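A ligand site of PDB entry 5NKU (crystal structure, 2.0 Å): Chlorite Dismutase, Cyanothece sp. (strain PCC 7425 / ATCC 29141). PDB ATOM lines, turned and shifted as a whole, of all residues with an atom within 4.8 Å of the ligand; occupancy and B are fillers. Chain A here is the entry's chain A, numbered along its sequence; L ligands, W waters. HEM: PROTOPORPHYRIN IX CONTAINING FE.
N of Phe 147 is in hydrogen-bond range of O of Ile 96 (3.0 Å). NZ of Lys 98 lies within salt-bridge range of OE2 of Glu 173 (2.6 Å). The side-chain hydroxyl (OG1) of Thr 149 is in hydrogen-bond range of the backbone carbonyl oxygen (O) of Ile 94 (2.7 Å). N of His 120 lies within hydrogen-bond range of O of Phe 114 (3.2 Å). A ring nitrogen (ND1) of His 120 is in hydrogen-bond range of the side-chain carboxylate of Glu 173. NE of Arg 66 is in hydrogen-bond range of O of Asn 64 (3.2 Å). The indole nitrogen of Trp 174 sits at hydrogen-bond distance from the side-chain carboxylate of Glu 180, 2.9 Å away.
Ile 65 touches the ligand. Leu 76 touches the ligand (CD1 to CMA, 3.6 Å). CD1 of Ile 94 touches CBC of the ligand (3.9 Å). CD1 of Ile 96 touches CMD of the ligand, 3.7 Å away. Trp 102 touches the ligand (CZ2 to O1D, 3.6 Å). Phe 114 touches the ligand (CZ to C2A, 3.4 Å). OG1 of Thr 121 touches CMA of the ligand (3.6 Å). O of Gly 124 touches CAB of the ligand, at 3.5 Å. Leu 128 touches the ligand. Val 131 touches the ligand. CD of Arg 133 touches C2B of the ligand, 3.6 Å away. Leu 135 touches the ligand (CD1 to C3D, 3.96 Å). CZ of Phe 147 touches CGD of the ligand (3.4 Å). Thr 149 touches the ligand (CG2 to CHD, 3.7 Å). Phe 151 touches the ligand. CD2 of Leu 164 touches CBB of the ligand, 3.4 Å away. Leu 165 touches the ligand. Met 168 touches the ligand (CE to C2C, 3.1 Å). Glu 173 touches the ligand. Trp 174 touches the ligand. Glu 180 touches the ligand. Hydrophobic or aromatic side chains that line the ligand: Ile 65, Tyr 67, Ala 68, Leu 76, Ile 94, Ile 96, Trp 102, Phe 114, His 120, Leu 128, Val 131, Leu 135, Phe 147, Phe 151, Leu 164, Leu 165, Met 168 and Trp 174. Within 4 Å of the ligand: Ile 65, Arg 66, Tyr 67, Ala 68, Leu 76, Ile 94, Ile 96, Lys 98, Trp 102, Phe 114, His 120, Thr 121, Gly 124, Leu 128, Val 131, Arg 133, Leu 135, Phe 147, Thr 149, Phe 151, Leu 164, Leu 165, Met 168, Glu 173, Trp 174 and Glu 180.
Water W2 lies within hydrogen-bond range of O1D of the ligand (2.6 Å), OH of Tyr 67 (2.6 Å) and NE1 of Trp 102 (2.9 Å). Water W3 lies within hydrogen-bond range of O of Asn 64 and O1A of the ligand.
N of Arg 66 sits at hydrogen-bond distance from O1A of the ligand (2.7 Å). The backbone NH (N) of Tyr 67 sits at hydrogen-bond distance from an oxygen (O2A) of the ligand (2.7 Å). N of Ala 68 is in hydrogen-bond range of O2A of the ligand. O1D of the ligand lies within salt-bridge range of NZ of Lys 98 (2.8 Å). FE of the ligand is bound by NE2 of His 120, at 2.1 Å.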
ATOM      1  N   ASN A  64      19.797   0.425 -31.555  1.00  0.00           N
ATOM      2  CA  ASN A  64      18.412   0.087 -31.331  1.00  0.00           C
ATOM      3  C   ASN A  64      17.856   0.830 -30.092  1.00  0.00           C
ATOM      4  O   ASN A  64      18.590   1.288 -29.242  1.00  0.00           O
ATOM      5  CB  ASN A  64      18.238  -1.432 -31.138  1.00  0.00           C
ATOM      6  CG  ASN A  64      19.145  -1.959 -29.977  1.00  0.00           C
ATOM      7  OD1 ASN A  64      20.346  -2.056 -30.083  1.00  0.00           O
ATOM      8  ND2 ASN A  64      18.520  -2.283 -28.884  1.00  0.00           N
ATOM      9  N   ILE A  65      16.535   0.856 -29.992  1.00  0.00           N
ATOM     10  CA  ILE A  65      15.856   1.343 -28.792  1.00  0.00           C
ATOM     11  C   ILE A  65      16.178   0.551 -27.547  1.00  0.00           C
ATOM     12  O   ILE A  65      16.168  -0.692 -27.548  1.00  0.00           O
ATOM     13  CB  ILE A  65      14.374   1.328 -29.135  1.00  0.00           C
ATOM     14  CG1 ILE A  65      14.100   2.362 -30.272  1.00  0.00           C
ATOM     15  CG2 ILE A  65      13.368   1.478 -27.923  1.00  0.00           C
ATOM     16  CD1 ILE A  65      14.054   3.779 -29.853  1.00  0.00           C
ATOM     17  N   ARG A  66      16.391   1.278 -26.464  1.00  0.00           N
ATOM     18  CA  ARG A  66      16.771   0.734 -25.179  1.00  0.00           C
ATOM     19  C   ARG A  66      15.690   0.861 -24.148  1.00  0.00           C
ATOM     20  O   ARG A  66      15.708   0.066 -23.221  1.00  0.00           O
ATOM     21  CB  ARG A  66      18.086   1.405 -24.616  1.00  0.00           C
ATOM     22  CG  ARG A  66      19.162   1.471 -25.648  1.00  0.00           C
ATOM     23  CD  ARG A  66      19.604   0.072 -26.162  1.00  0.00           C
ATOM     24  NE  ARG A  66      20.738   0.150 -27.108  1.00  0.00           N
ATOM     25  CZ  ARG A  66      22.019   0.235 -26.757  1.00  0.00           C
ATOM     26  NH1 ARG A  66      22.359   0.178 -25.479  1.00  0.00           N
ATOM     27  NH2 ARG A  66      22.919   0.306 -27.667  1.00  0.00           N
ATOM     28  N   TYR A  67      14.721   1.789 -24.304  1.00  0.00           N
ATOM     29  CA  TYR A  67      13.772   2.133 -23.231  1.00  0.00           C
ATOM     30  C   TYR A  67      12.370   2.312 -23.774  1.00  0.00           C
ATOM     31  O   TYR A  67      11.397   1.897 -23.141  1.00  0.00           O
ATOM     32  CB  TYR A  67      14.204   3.427 -22.440  1.00  0.00           C
ATOM     33  CG  TYR A  67      15.410   3.223 -21.633  1.00  0.00           C
ATOM     34  CD1 TYR A  67      15.381   2.319 -20.550  1.00  0.00           C
ATOM     35  CD2 TYR A  67      16.606   3.800 -21.992  1.00  0.00           C
ATOM     36  CE1 TYR A  67      16.541   2.068 -19.818  1.00  0.00           C
ATOM     37  CE2 TYR A  67      17.838   3.479 -21.313  1.00  0.00           C
ATOM     38  CZ  TYR A  67      17.785   2.638 -20.174  1.00  0.00           C
ATOM     39  OH  TYR A  67      18.937   2.398 -19.432  1.00  0.00           O
ATOM     40  N   ALA A  68      12.200   2.990 -24.898  1.00  0.00           N
ATOM     41  CA  ALA A  68      10.842   3.373 -25.313  1.00  0.00           C
ATOM     42  C   ALA A  68       9.990   2.130 -25.499  1.00  0.00           C
ATOM     43  O   ALA A  68      10.479   1.143 -26.030  1.00  0.00           O
ATOM     44  CB  ALA A  68      10.919   4.140 -26.612  1.00  0.00           C
ATOM     45  N   LEU A  76       5.899   9.442 -30.647  1.00  0.00           N
ATOM     46  CA  LEU A  76       7.093  10.105 -31.151  1.00  0.00           C
ATOM     47  C   LEU A  76       7.064  10.117 -32.647  1.00  0.00           C
ATOM     48  O   LEU A  76       7.357  11.124 -33.294  1.00  0.00           O
ATOM     49  CB  LEU A  76       8.335   9.329 -30.694  1.00  0.00           C
ATOM     50  CG  LEU A  76       8.717   9.621 -29.234  1.00  0.00           C
ATOM     51  CD1 LEU A  76       9.631   8.528 -28.555  1.00  0.00           C
ATOM     52  CD2 LEU A  76       9.406  10.902 -29.226  1.00  0.00           C
ATOM     53  N   ILE A  94      25.102  17.888 -27.374  1.00  0.00           N
ATOM     54  CA  ILE A  94      25.250  17.745 -25.927  1.00  0.00           C
ATOM     55  C   ILE A  94      25.804  16.366 -25.614  1.00  0.00           C
ATOM     56  O   ILE A  94      25.030  15.389 -25.429  1.00  0.00           O
ATOM     57  CB  ILE A  94      23.942  18.017 -25.162  1.00  0.00           C
ATOM     58  CG1 ILE A  94      23.385  19.393 -25.626  1.00  0.00           C
ATOM     59  CG2 ILE A  94      24.194  18.013 -23.575  1.00  0.00           C
ATOM     60  CD1 ILE A  94      22.107  19.794 -24.899  1.00  0.00           C
ATOM     61  N   ILE A  96      27.063  13.675 -23.026  1.00  0.00           N
ATOM     62  CA  ILE A  96      26.634  13.327 -21.671  1.00  0.00           C
ATOM     63  C   ILE A  96      27.330  12.044 -21.184  1.00  0.00           C
ATOM     64  O   ILE A  96      27.540  11.111 -21.974  1.00  0.00           O
ATOM     65  CB  ILE A  96      25.110  13.133 -21.660  1.00  0.00           C
ATOM     66  CG1 ILE A  96      24.406  14.535 -21.595  1.00  0.00           C
ATOM     67  CG2 ILE A  96      24.676  12.386 -20.434  1.00  0.00           C
ATOM     68  CD1 ILE A  96      22.974  14.528 -21.929  1.00  0.00           C
ATOM     69  N   LYS A  98      26.987   9.337 -17.832  1.00  0.00           N
ATOM     70  CA  LYS A  98      26.323   8.970 -16.592  1.00  0.00           C
ATOM     71  C   LYS A  98      27.282   8.208 -15.688  1.00  0.00           C
ATOM     72  O   LYS A  98      28.257   7.595 -16.122  1.00  0.00           O
ATOM     73  CB  LYS A  98      25.076   8.139 -16.887  1.00  0.00           C
ATOM     74  CG  LYS A  98      23.957   8.990 -17.620  1.00  0.00           C
ATOM     75  CD  LYS A  98      22.651   8.185 -17.766  1.00  0.00           C
ATOM     76  CE  LYS A  98      21.513   8.884 -18.553  1.00  0.00           C
ATOM     77  NZ  LYS A  98      20.153   8.253 -18.462  1.00  0.00           N
ATOM     78  N   TRP A 102      24.731   4.321 -12.372  1.00  0.00           N
ATOM     79  CA  TRP A 102      23.640   4.162 -13.312  1.00  0.00           C
ATOM     80  C   TRP A 102      23.765   2.849 -14.082  1.00  0.00           C
ATOM     81  O   TRP A 102      22.792   2.152 -14.285  1.00  0.00           O
ATOM     82  CB  TRP A 102      23.619   5.342 -14.292  1.00  0.00           C
ATOM     83  CG  TRP A 102      22.673   5.172 -15.492  1.00  0.00           C
ATOM     84  CD1 TRP A 102      23.003   4.806 -16.729  1.00  0.00           C
ATOM     85  CD2 TRP A 102      21.261   5.409 -15.502  1.00  0.00           C
ATOM     86  NE1 TRP A 102      21.886   4.735 -17.528  1.00  0.00           N
ATOM     87  CE2 TRP A 102      20.803   5.140 -16.803  1.00  0.00           C
ATOM     88  CE3 TRP A 102      20.335   5.826 -14.533  1.00  0.00           C
ATOM     89  CZ2 TRP A 102      19.492   5.274 -17.153  1.00  0.00           C
ATOM     90  CZ3 TRP A 102      19.031   5.948 -14.894  1.00  0.00           C
ATOM     91  CH2 TRP A 102      18.617   5.676 -16.179  1.00  0.00           C
ATOM     92  N   PHE A 114      14.033   6.503 -15.789  1.00  0.00           N
ATOM     93  CA  PHE A 114      14.039   7.206 -17.047  1.00  0.00           C
ATOM     94  C   PHE A 114      12.658   7.790 -17.349  1.00  0.00           C
ATOM     95  O   PHE A 114      12.524   8.957 -17.749  1.00  0.00           O
ATOM     96  CB  PHE A 114      14.489   6.285 -18.190  1.00  0.00           C
ATOM     97  CG  PHE A 114      14.408   6.878 -19.549  1.00  0.00           C
ATOM     98  CD1 PHE A 114      15.414   7.764 -20.024  1.00  0.00           C
ATOM     99  CD2 PHE A 114      13.333   6.621 -20.321  1.00  0.00           C
ATOM    100  CE1 PHE A 114      15.360   8.318 -21.283  1.00  0.00           C
ATOM    101  CE2 PHE A 114      13.245   7.193 -21.594  1.00  0.00           C
ATOM    102  CZ  PHE A 114      14.243   8.055 -22.068  1.00  0.00           C
ATOM    103  N   HIS A 120      11.055  11.415 -19.117  1.00  0.00           N
ATOM    104  CA  HIS A 120      11.913  11.904 -20.184  1.00  0.00           C
ATOM    105  C   HIS A 120      11.139  12.026 -21.456  1.00  0.00           C
ATOM    106  O   HIS A 120      11.205  13.052 -22.132  1.00  0.00           O
ATOM    107  CB  HIS A 120      13.127  10.970 -20.375  1.00  0.00           C
ATOM    108  CG  HIS A 120      14.228  11.493 -21.288  1.00  0.00           C
ATOM    109  ND1 HIS A 120      15.502  11.641 -20.830  1.00  0.00           N
ATOM    110  CD2 HIS A 120      14.279  11.836 -22.599  1.00  0.00           C
ATOM    111  CE1 HIS A 120      16.301  12.033 -21.799  1.00  0.00           C
ATOM    112  NE2 HIS A 120      15.587  12.118 -22.892  1.00  0.00           N
ATOM    113  N   THR A 121      10.393  11.000 -21.792  1.00  0.00           N
ATOM    114  CA  THR A 121       9.803  10.988 -23.119  1.00  0.00           C
ATOM    115  C   THR A 121       8.595  11.901 -23.150  1.00  0.00           C
ATOM    116  O   THR A 121       8.411  12.692 -24.065  1.00  0.00           O
ATOM    117  CB  THR A 121       9.422   9.559 -23.502  1.00  0.00           C
ATOM    118  OG1 THR A 121      10.597   8.737 -23.423  1.00  0.00           O
ATOM    119  CG2 THR A 121       8.832   9.528 -24.856  1.00  0.00           C
ATOM    120  N   GLY A 124       9.765  15.517 -23.181  1.00  0.00           N
ATOM    121  CA  GLY A 124      10.397  15.886 -24.454  1.00  0.00           C
ATOM    122  C   GLY A 124       9.364  16.025 -25.546  1.00  0.00           C
ATOM    123  O   GLY A 124       9.450  16.921 -26.426  1.00  0.00           O
ATOM    124  N   LEU A 125       8.317  15.195 -25.461  1.00  0.00           N
ATOM    125  CA  LEU A 125       7.318  15.196 -26.506  1.00  0.00           C
ATOM    126  C   LEU A 125       6.599  16.535 -26.526  1.00  0.00           C
ATOM    127  O   LEU A 125       6.041  16.910 -27.574  1.00  0.00           O
ATOM    128  CB  LEU A 125       6.345  14.056 -26.221  1.00  0.00           C
ATOM    129  CG  LEU A 125       5.844  13.130 -27.313  1.00  0.00           C
ATOM    130  CD1 LEU A 125       6.832  12.734 -28.309  1.00  0.00           C
ATOM    131  CD2 LEU A 125       5.438  11.868 -26.602  1.00  0.00           C
ATOM    132  N   LEU A 128       8.304  18.655 -29.384  1.00  0.00           N
ATOM    133  CA  LEU A 128       8.155  18.344 -30.783  1.00  0.00           C
ATOM    134  C   LEU A 128       6.909  19.049 -31.327  1.00  0.00           C
ATOM    135  O   LEU A 128       5.985  19.320 -30.559  1.00  0.00           O
ATOM    136  CB  LEU A 128       8.035  16.868 -30.937  1.00  0.00           C
ATOM    137  CG  LEU A 128       9.364  16.291 -30.997  1.00  0.00           C
ATOM    138  CD1 LEU A 128      10.300  16.725 -29.851  1.00  0.00           C
ATOM    139  CD2 LEU A 128       9.256  14.743 -31.004  1.00  0.00           C
ATOM    140  N   VAL A 131      11.691  20.836 -31.984  1.00  0.00           N
ATOM    141  CA  VAL A 131      13.022  20.285 -31.889  1.00  0.00           C
ATOM    142  C   VAL A 131      13.080  18.969 -32.635  1.00  0.00           C
ATOM    143  O   VAL A 131      12.340  18.032 -32.316  1.00  0.00           O
ATOM    144  CB  VAL A 131      13.437  20.115 -30.405  1.00  0.00           C
ATOM    145  CG1 VAL A 131      14.817  19.519 -30.253  1.00  0.00           C
ATOM    146  CG2 VAL A 131      13.453  21.438 -29.710  1.00  0.00           C
ATOM    147  N   ARG A 133      15.719  15.636 -33.256  1.00  0.00           N
ATOM    148  CA  ARG A 133      16.786  15.077 -32.437  1.00  0.00           C
ATOM    149  C   ARG A 133      17.392  13.800 -33.040  1.00  0.00           C
ATOM    150  O   ARG A 133      16.739  13.059 -33.755  1.00  0.00           O
ATOM    151  CB  ARG A 133      16.261  14.796 -31.052  1.00  0.00           C
ATOM    152  CG  ARG A 133      15.293  13.719 -31.074  1.00  0.00           C
ATOM    153  CD  ARG A 133      14.770  13.406 -29.651  1.00  0.00           C
ATOM    154  NE  ARG A 133      14.287  12.052 -29.680  1.00  0.00           N
ATOM    155  CZ  ARG A 133      13.256  11.657 -30.448  1.00  0.00           C
ATOM    156  NH1 ARG A 133      12.528  12.493 -31.271  1.00  0.00           N
ATOM    157  NH2 ARG A 133      12.937  10.403 -30.386  1.00  0.00           N
ATOM    158  N   LEU A 135      20.096  10.598 -31.321  1.00  0.00           N
ATOM    159  CA  LEU A 135      20.781  10.023 -30.197  1.00  0.00           C
ATOM    160  C   LEU A 135      21.877   9.095 -30.682  1.00  0.00           C
ATOM    161  O   LEU A 135      21.613   8.176 -31.448  1.00  0.00           O
ATOM    162  CB  LEU A 135      19.788   9.244 -29.342  1.00  0.00           C
ATOM    163  CG  LEU A 135      20.484   8.476 -28.186  1.00  0.00           C
ATOM    164  CD1 LEU A 135      21.064   9.388 -27.187  1.00  0.00           C
ATOM    165  CD2 LEU A 135      19.392   7.610 -27.447  1.00  0.00           C
ATOM    166  N   PHE A 147      26.965   9.318 -24.323  1.00  0.00           N
ATOM    167  CA  PHE A 147      25.977   9.655 -25.346  1.00  0.00           C
ATOM    168  C   PHE A 147      26.397  10.951 -26.066  1.00  0.00           C
ATOM    169  O   PHE A 147      27.037  11.806 -25.468  1.00  0.00           O
ATOM    170  CB  PHE A 147      24.605   9.820 -24.765  1.00  0.00           C
ATOM    171  CG  PHE A 147      24.119   8.664 -23.944  1.00  0.00           C
ATOM    172  CD1 PHE A 147      23.656   7.560 -24.576  1.00  0.00           C
ATOM    173  CD2 PHE A 147      24.117   8.727 -22.527  1.00  0.00           C
ATOM    174  CE1 PHE A 147      23.203   6.464 -23.846  1.00  0.00           C
ATOM    175  CE2 PHE A 147      23.659   7.611 -21.749  1.00  0.00           C
ATOM    176  CZ  PHE A 147      23.261   6.507 -22.450  1.00  0.00           C
ATOM    177  N   THR A 149      24.112  13.626 -28.055  1.00  0.00           N
ATOM    178  CA  THR A 149      22.762  14.041 -28.404  1.00  0.00           C
ATOM    179  C   THR A 149      22.820  15.281 -29.269  1.00  0.00           C
ATOM    180  O   THR A 149      23.660  16.158 -29.093  1.00  0.00           O
ATOM    181  CB  THR A 149      21.917  14.300 -27.104  1.00  0.00           C
ATOM    182  OG1 THR A 149      22.473  15.378 -26.289  1.00  0.00           O
ATOM    183  CG2 THR A 149      21.784  13.069 -26.206  1.00  0.00           C
ATOM    184  N   PHE A 151      20.403  18.157 -31.464  1.00  0.00           N
ATOM    185  CA  PHE A 151      19.105  18.822 -31.471  1.00  0.00           C
ATOM    186  C   PHE A 151      19.224  19.943 -32.504  1.00  0.00           C
ATOM    187  O   PHE A 151      20.262  20.609 -32.584  1.00  0.00           O
ATOM    188  CB  PHE A 151      18.708  19.376 -30.080  1.00  0.00           C
ATOM    189  CG  PHE A 151      18.681  18.310 -29.032  1.00  0.00           C
ATOM    190  CD1 PHE A 151      17.592  17.496 -28.957  1.00  0.00           C
ATOM    191  CD2 PHE A 151      19.769  18.144 -28.160  1.00  0.00           C
ATOM    192  CE1 PHE A 151      17.586  16.459 -28.053  1.00  0.00           C
ATOM    193  CE2 PHE A 151      19.820  17.159 -27.284  1.00  0.00           C
ATOM    194  CZ  PHE A 151      18.721  16.274 -27.183  1.00  0.00           C
ATOM    195  N   PHE A 161      13.664  25.479 -26.305  1.00  0.00           N
ATOM    196  CA  PHE A 161      14.723  24.487 -26.129  1.00  0.00           C
ATOM    197  C   PHE A 161      15.420  24.677 -24.790  1.00  0.00           C
ATOM    198  O   PHE A 161      15.706  23.719 -24.067  1.00  0.00           O
ATOM    199  CB  PHE A 161      15.748  24.524 -27.279  1.00  0.00           C
ATOM    200  CG  PHE A 161      16.752  23.397 -27.171  1.00  0.00           C
ATOM    201  CD1 PHE A 161      16.359  22.075 -27.403  1.00  0.00           C
ATOM    202  CD2 PHE A 161      18.047  23.621 -26.697  1.00  0.00           C
ATOM    203  CE1 PHE A 161      17.210  20.989 -27.250  1.00  0.00           C
ATOM    204  CE2 PHE A 161      18.949  22.585 -26.544  1.00  0.00           C
ATOM    205  CZ  PHE A 161      18.530  21.246 -26.804  1.00  0.00           C
ATOM    206  N   LEU A 164      13.166  23.336 -21.891  1.00  0.00           N
ATOM    207  CA  LEU A 164      13.329  21.877 -21.844  1.00  0.00           C
ATOM    208  C   LEU A 164      14.575  21.484 -21.055  1.00  0.00           C
ATOM    209  O   LEU A 164      14.546  20.558 -20.226  1.00  0.00           O
ATOM    210  CB  LEU A 164      13.397  21.344 -23.262  1.00  0.00           C
ATOM    211  CG  LEU A 164      13.737  19.834 -23.386  1.00  0.00           C
ATOM    212  CD1 LEU A 164      12.659  18.864 -22.897  1.00  0.00           C
ATOM    213  CD2 LEU A 164      13.984  19.629 -24.836  1.00  0.00           C
ATOM    214  N   LEU A 165      15.681  22.189 -21.294  1.00  0.00           N
ATOM    215  CA  LEU A 165      16.936  21.762 -20.664  1.00  0.00           C
ATOM    216  C   LEU A 165      16.877  21.939 -19.174  1.00  0.00           C
ATOM    217  O   LEU A 165      17.332  21.058 -18.437  1.00  0.00           O
ATOM    218  CB  LEU A 165      18.136  22.528 -21.194  1.00  0.00           C
ATOM    219  CG  LEU A 165      18.596  22.360 -22.706  1.00  0.00           C
ATOM    220  CD1 LEU A 165      19.773  23.234 -23.105  1.00  0.00           C
ATOM    221  CD2 LEU A 165      18.881  20.906 -23.058  1.00  0.00           C
ATOM    222  N   MET A 168      14.658  19.064 -17.839  1.00  0.00           N
ATOM    223  CA  MET A 168      15.291  17.776 -17.776  1.00  0.00           C
ATOM    224  C   MET A 168      16.389  17.748 -16.706  1.00  0.00           C
ATOM    225  O   MET A 168      16.523  16.769 -15.970  1.00  0.00           O
ATOM    226  CB  MET A 168      15.790  17.435 -19.180  1.00  0.00           C
ATOM    227  CG  MET A 168      15.544  15.910 -19.551  1.00  0.00           C
ATOM    228  SD  MET A 168      14.383  15.531 -20.899  1.00  0.00           S
ATOM    229  CE  MET A 168      15.222  16.621 -21.974  1.00  0.00           C
ATOM    230  N   GLU A 173      16.586  11.481 -13.267  1.00  0.00           N
ATOM    231  CA  GLU A 173      17.559  10.923 -14.207  1.00  0.00           C
ATOM    232  C   GLU A 173      18.829  11.713 -14.109  1.00  0.00           C
ATOM    233  O   GLU A 173      19.926  11.168 -14.225  1.00  0.00           O
ATOM    234  CB  GLU A 173      17.057  11.032 -15.657  1.00  0.00           C
ATOM    235  CG  GLU A 173      18.030  10.324 -16.697  1.00  0.00           C
ATOM    236  CD  GLU A 173      17.565  10.406 -18.129  1.00  0.00           C
ATOM    237  OE1 GLU A 173      16.521  11.037 -18.330  1.00  0.00           O
ATOM    238  OE2 GLU A 173      18.234   9.886 -19.067  1.00  0.00           O
ATOM    239  N   TRP A 174      18.713  13.035 -14.045  1.00  0.00           N
ATOM    240  CA  TRP A 174      19.921  13.871 -14.130  1.00  0.00           C
ATOM    241  C   TRP A 174      20.786  13.820 -12.862  1.00  0.00           C
ATOM    242  O   TRP A 174      21.944  14.250 -12.871  1.00  0.00           O
ATOM    243  CB  TRP A 174      19.571  15.333 -14.448  1.00  0.00           C
ATOM    244  CG  TRP A 174      20.133  15.687 -15.812  1.00  0.00           C
ATOM    245  CD1 TRP A 174      21.221  16.462 -16.086  1.00  0.00           C
ATOM    246  CD2 TRP A 174      19.646  15.245 -17.044  1.00  0.00           C
ATOM    247  NE1 TRP A 174      21.419  16.547 -17.426  1.00  0.00           N
ATOM    248  CE2 TRP A 174      20.470  15.790 -18.035  1.00  0.00           C
ATOM    249  CE3 TRP A 174      18.583  14.436 -17.417  1.00  0.00           C
ATOM    250  CZ2 TRP A 174      20.279  15.546 -19.347  1.00  0.00           C
ATOM    251  CZ3 TRP A 174      18.400  14.174 -18.761  1.00  0.00           C
ATOM    252  CH2 TRP A 174      19.225  14.729 -19.684  1.00  0.00           C
ATOM    253  N   GLU A 180      28.595  16.905 -18.598  1.00  0.00           N
ATOM    254  CA  GLU A 180      27.676  17.475 -19.604  1.00  0.00           C
ATOM    255  C   GLU A 180      28.257  18.777 -20.178  1.00  0.00           C
ATOM    256  O   GLU A 180      28.775  19.589 -19.416  1.00  0.00           O
ATOM    257  CB  GLU A 180      26.312  17.746 -19.003  1.00  0.00           C
ATOM    258  CG  GLU A 180      25.267  18.135 -20.010  1.00  0.00           C
ATOM    259  CD  GLU A 180      23.908  18.276 -19.413  1.00  0.00           C
ATOM    260  OE1 GLU A 180      23.783  18.125 -18.187  1.00  0.00           O
ATOM    261  OE2 GLU A 180      22.951  18.598 -20.156  1.00  0.00           O
HETATM  262  CHA HEM L   1      17.109   9.183 -24.524  1.00  0.00           C
HETATM  263  CHB HEM L   1      13.220  11.352 -26.333  1.00  0.00           C
HETATM  264  CHC HEM L   1      15.341  15.420 -25.246  1.00  0.00           C
HETATM  265  CHD HEM L   1      19.330  13.329 -23.425  1.00  0.00           C
HETATM  266  C1A HEM L   1      15.867   9.407 -25.081  1.00  0.00           C
HETATM  267  C2A HEM L   1      14.973   8.357 -25.417  1.00  0.00           C
HETATM  268  C3A HEM L   1      13.851   8.952 -25.912  1.00  0.00           C
HETATM  269  C4A HEM L   1      14.079  10.388 -25.927  1.00  0.00           C
HETATM  270  CMA HEM L   1      12.521   8.329 -26.406  1.00  0.00           C
HETATM  271  CAA HEM L   1      15.212   6.847 -25.143  1.00  0.00           C
HETATM  272  CBA HEM L   1      15.623   6.132 -26.468  1.00  0.00           C
HETATM  273  CGA HEM L   1      15.717   4.609 -26.273  1.00  0.00           C
HETATM  274  O1A HEM L   1      16.814   3.965 -26.537  1.00  0.00           O
HETATM  275  O2A HEM L   1      14.714   3.964 -25.979  1.00  0.00           O
HETATM  276  C1B HEM L   1      13.483  12.678 -26.207  1.00  0.00           C
HETATM  277  C2B HEM L   1      12.668  13.741 -26.800  1.00  0.00           C
HETATM  278  C3B HEM L   1      13.295  14.869 -26.549  1.00  0.00           C
HETATM  279  C4B HEM L   1      14.479  14.547 -25.750  1.00  0.00           C
HETATM  280  CMB HEM L   1      11.379  13.457 -27.588  1.00  0.00           C
HETATM  281  CAB HEM L   1      12.828  16.264 -26.971  1.00  0.00           C
HETATM  282  CBB HEM L   1      13.728  17.217 -27.184  1.00  0.00           C
HETATM  283  C1C HEM L   1      16.545  15.223 -24.670  1.00  0.00           C
HETATM  284  C2C HEM L   1      17.386  16.275 -24.200  1.00  0.00           C
HETATM  285  C3C HEM L   1      18.534  15.712 -23.733  1.00  0.00           C
HETATM  286  C4C HEM L   1      18.391  14.284 -23.812  1.00  0.00           C
HETATM  287  CMC HEM L   1      17.231  17.802 -24.319  1.00  0.00           C
HETATM  288  CAC HEM L   1      19.812  16.260 -23.144  1.00  0.00           C
HETATM  289  CBC HEM L   1      20.096  17.365 -22.543  1.00  0.00           C
HETATM  290  C1D HEM L   1      19.124  11.960 -23.644  1.00  0.00           C
HETATM  291  C2D HEM L   1      20.021  10.833 -23.315  1.00  0.00           C
HETATM  292  C3D HEM L   1      19.389   9.710 -23.615  1.00  0.00           C
HETATM  293  C4D HEM L   1      18.073  10.074 -24.103  1.00  0.00           C
HETATM  294  CMD HEM L   1      21.386  11.236 -22.752  1.00  0.00           C
HETATM  295  CAD HEM L   1      19.829   8.290 -23.433  1.00  0.00           C
HETATM  296  CBD HEM L   1      19.512   7.951 -21.980  1.00  0.00           C
HETATM  297  CGD HEM L   1      19.962   6.516 -21.640  1.00  0.00           C
HETATM  298  O1D HEM L   1      20.421   6.290 -20.502  1.00  0.00           O
HETATM  299  O2D HEM L   1      19.981   5.620 -22.473  1.00  0.00           O
HETATM  300  NA  HEM L   1      15.283  10.686 -25.369  1.00  0.00           N
HETATM  301  NB  HEM L   1      14.545  13.192 -25.581  1.00  0.00           N
HETATM  302  NC  HEM L   1      17.166  13.968 -24.411  1.00  0.00           N
HETATM  303  ND  HEM L   1      18.035  11.435 -24.096  1.00  0.00           N
HETATM  304 FE   HEM L   1      16.243  12.288 -24.857  1.00  0.00          FE
HETATM  305  O   HOH W   1      21.468   3.000 -22.869  1.00  0.00           O
HETATM  306  O   HOH W   2      21.032   3.817 -20.158  1.00  0.00           O
HETATM  307  O   HOH W   3      18.726   4.036 -28.634  1.00  0.00           O
HETATM  308  O   HOH W   4      19.005   5.289 -25.090  1.00  0.00           O
HETATM  309  O   HOH W   5      15.860  10.194 -28.778  1.00  0.00           O
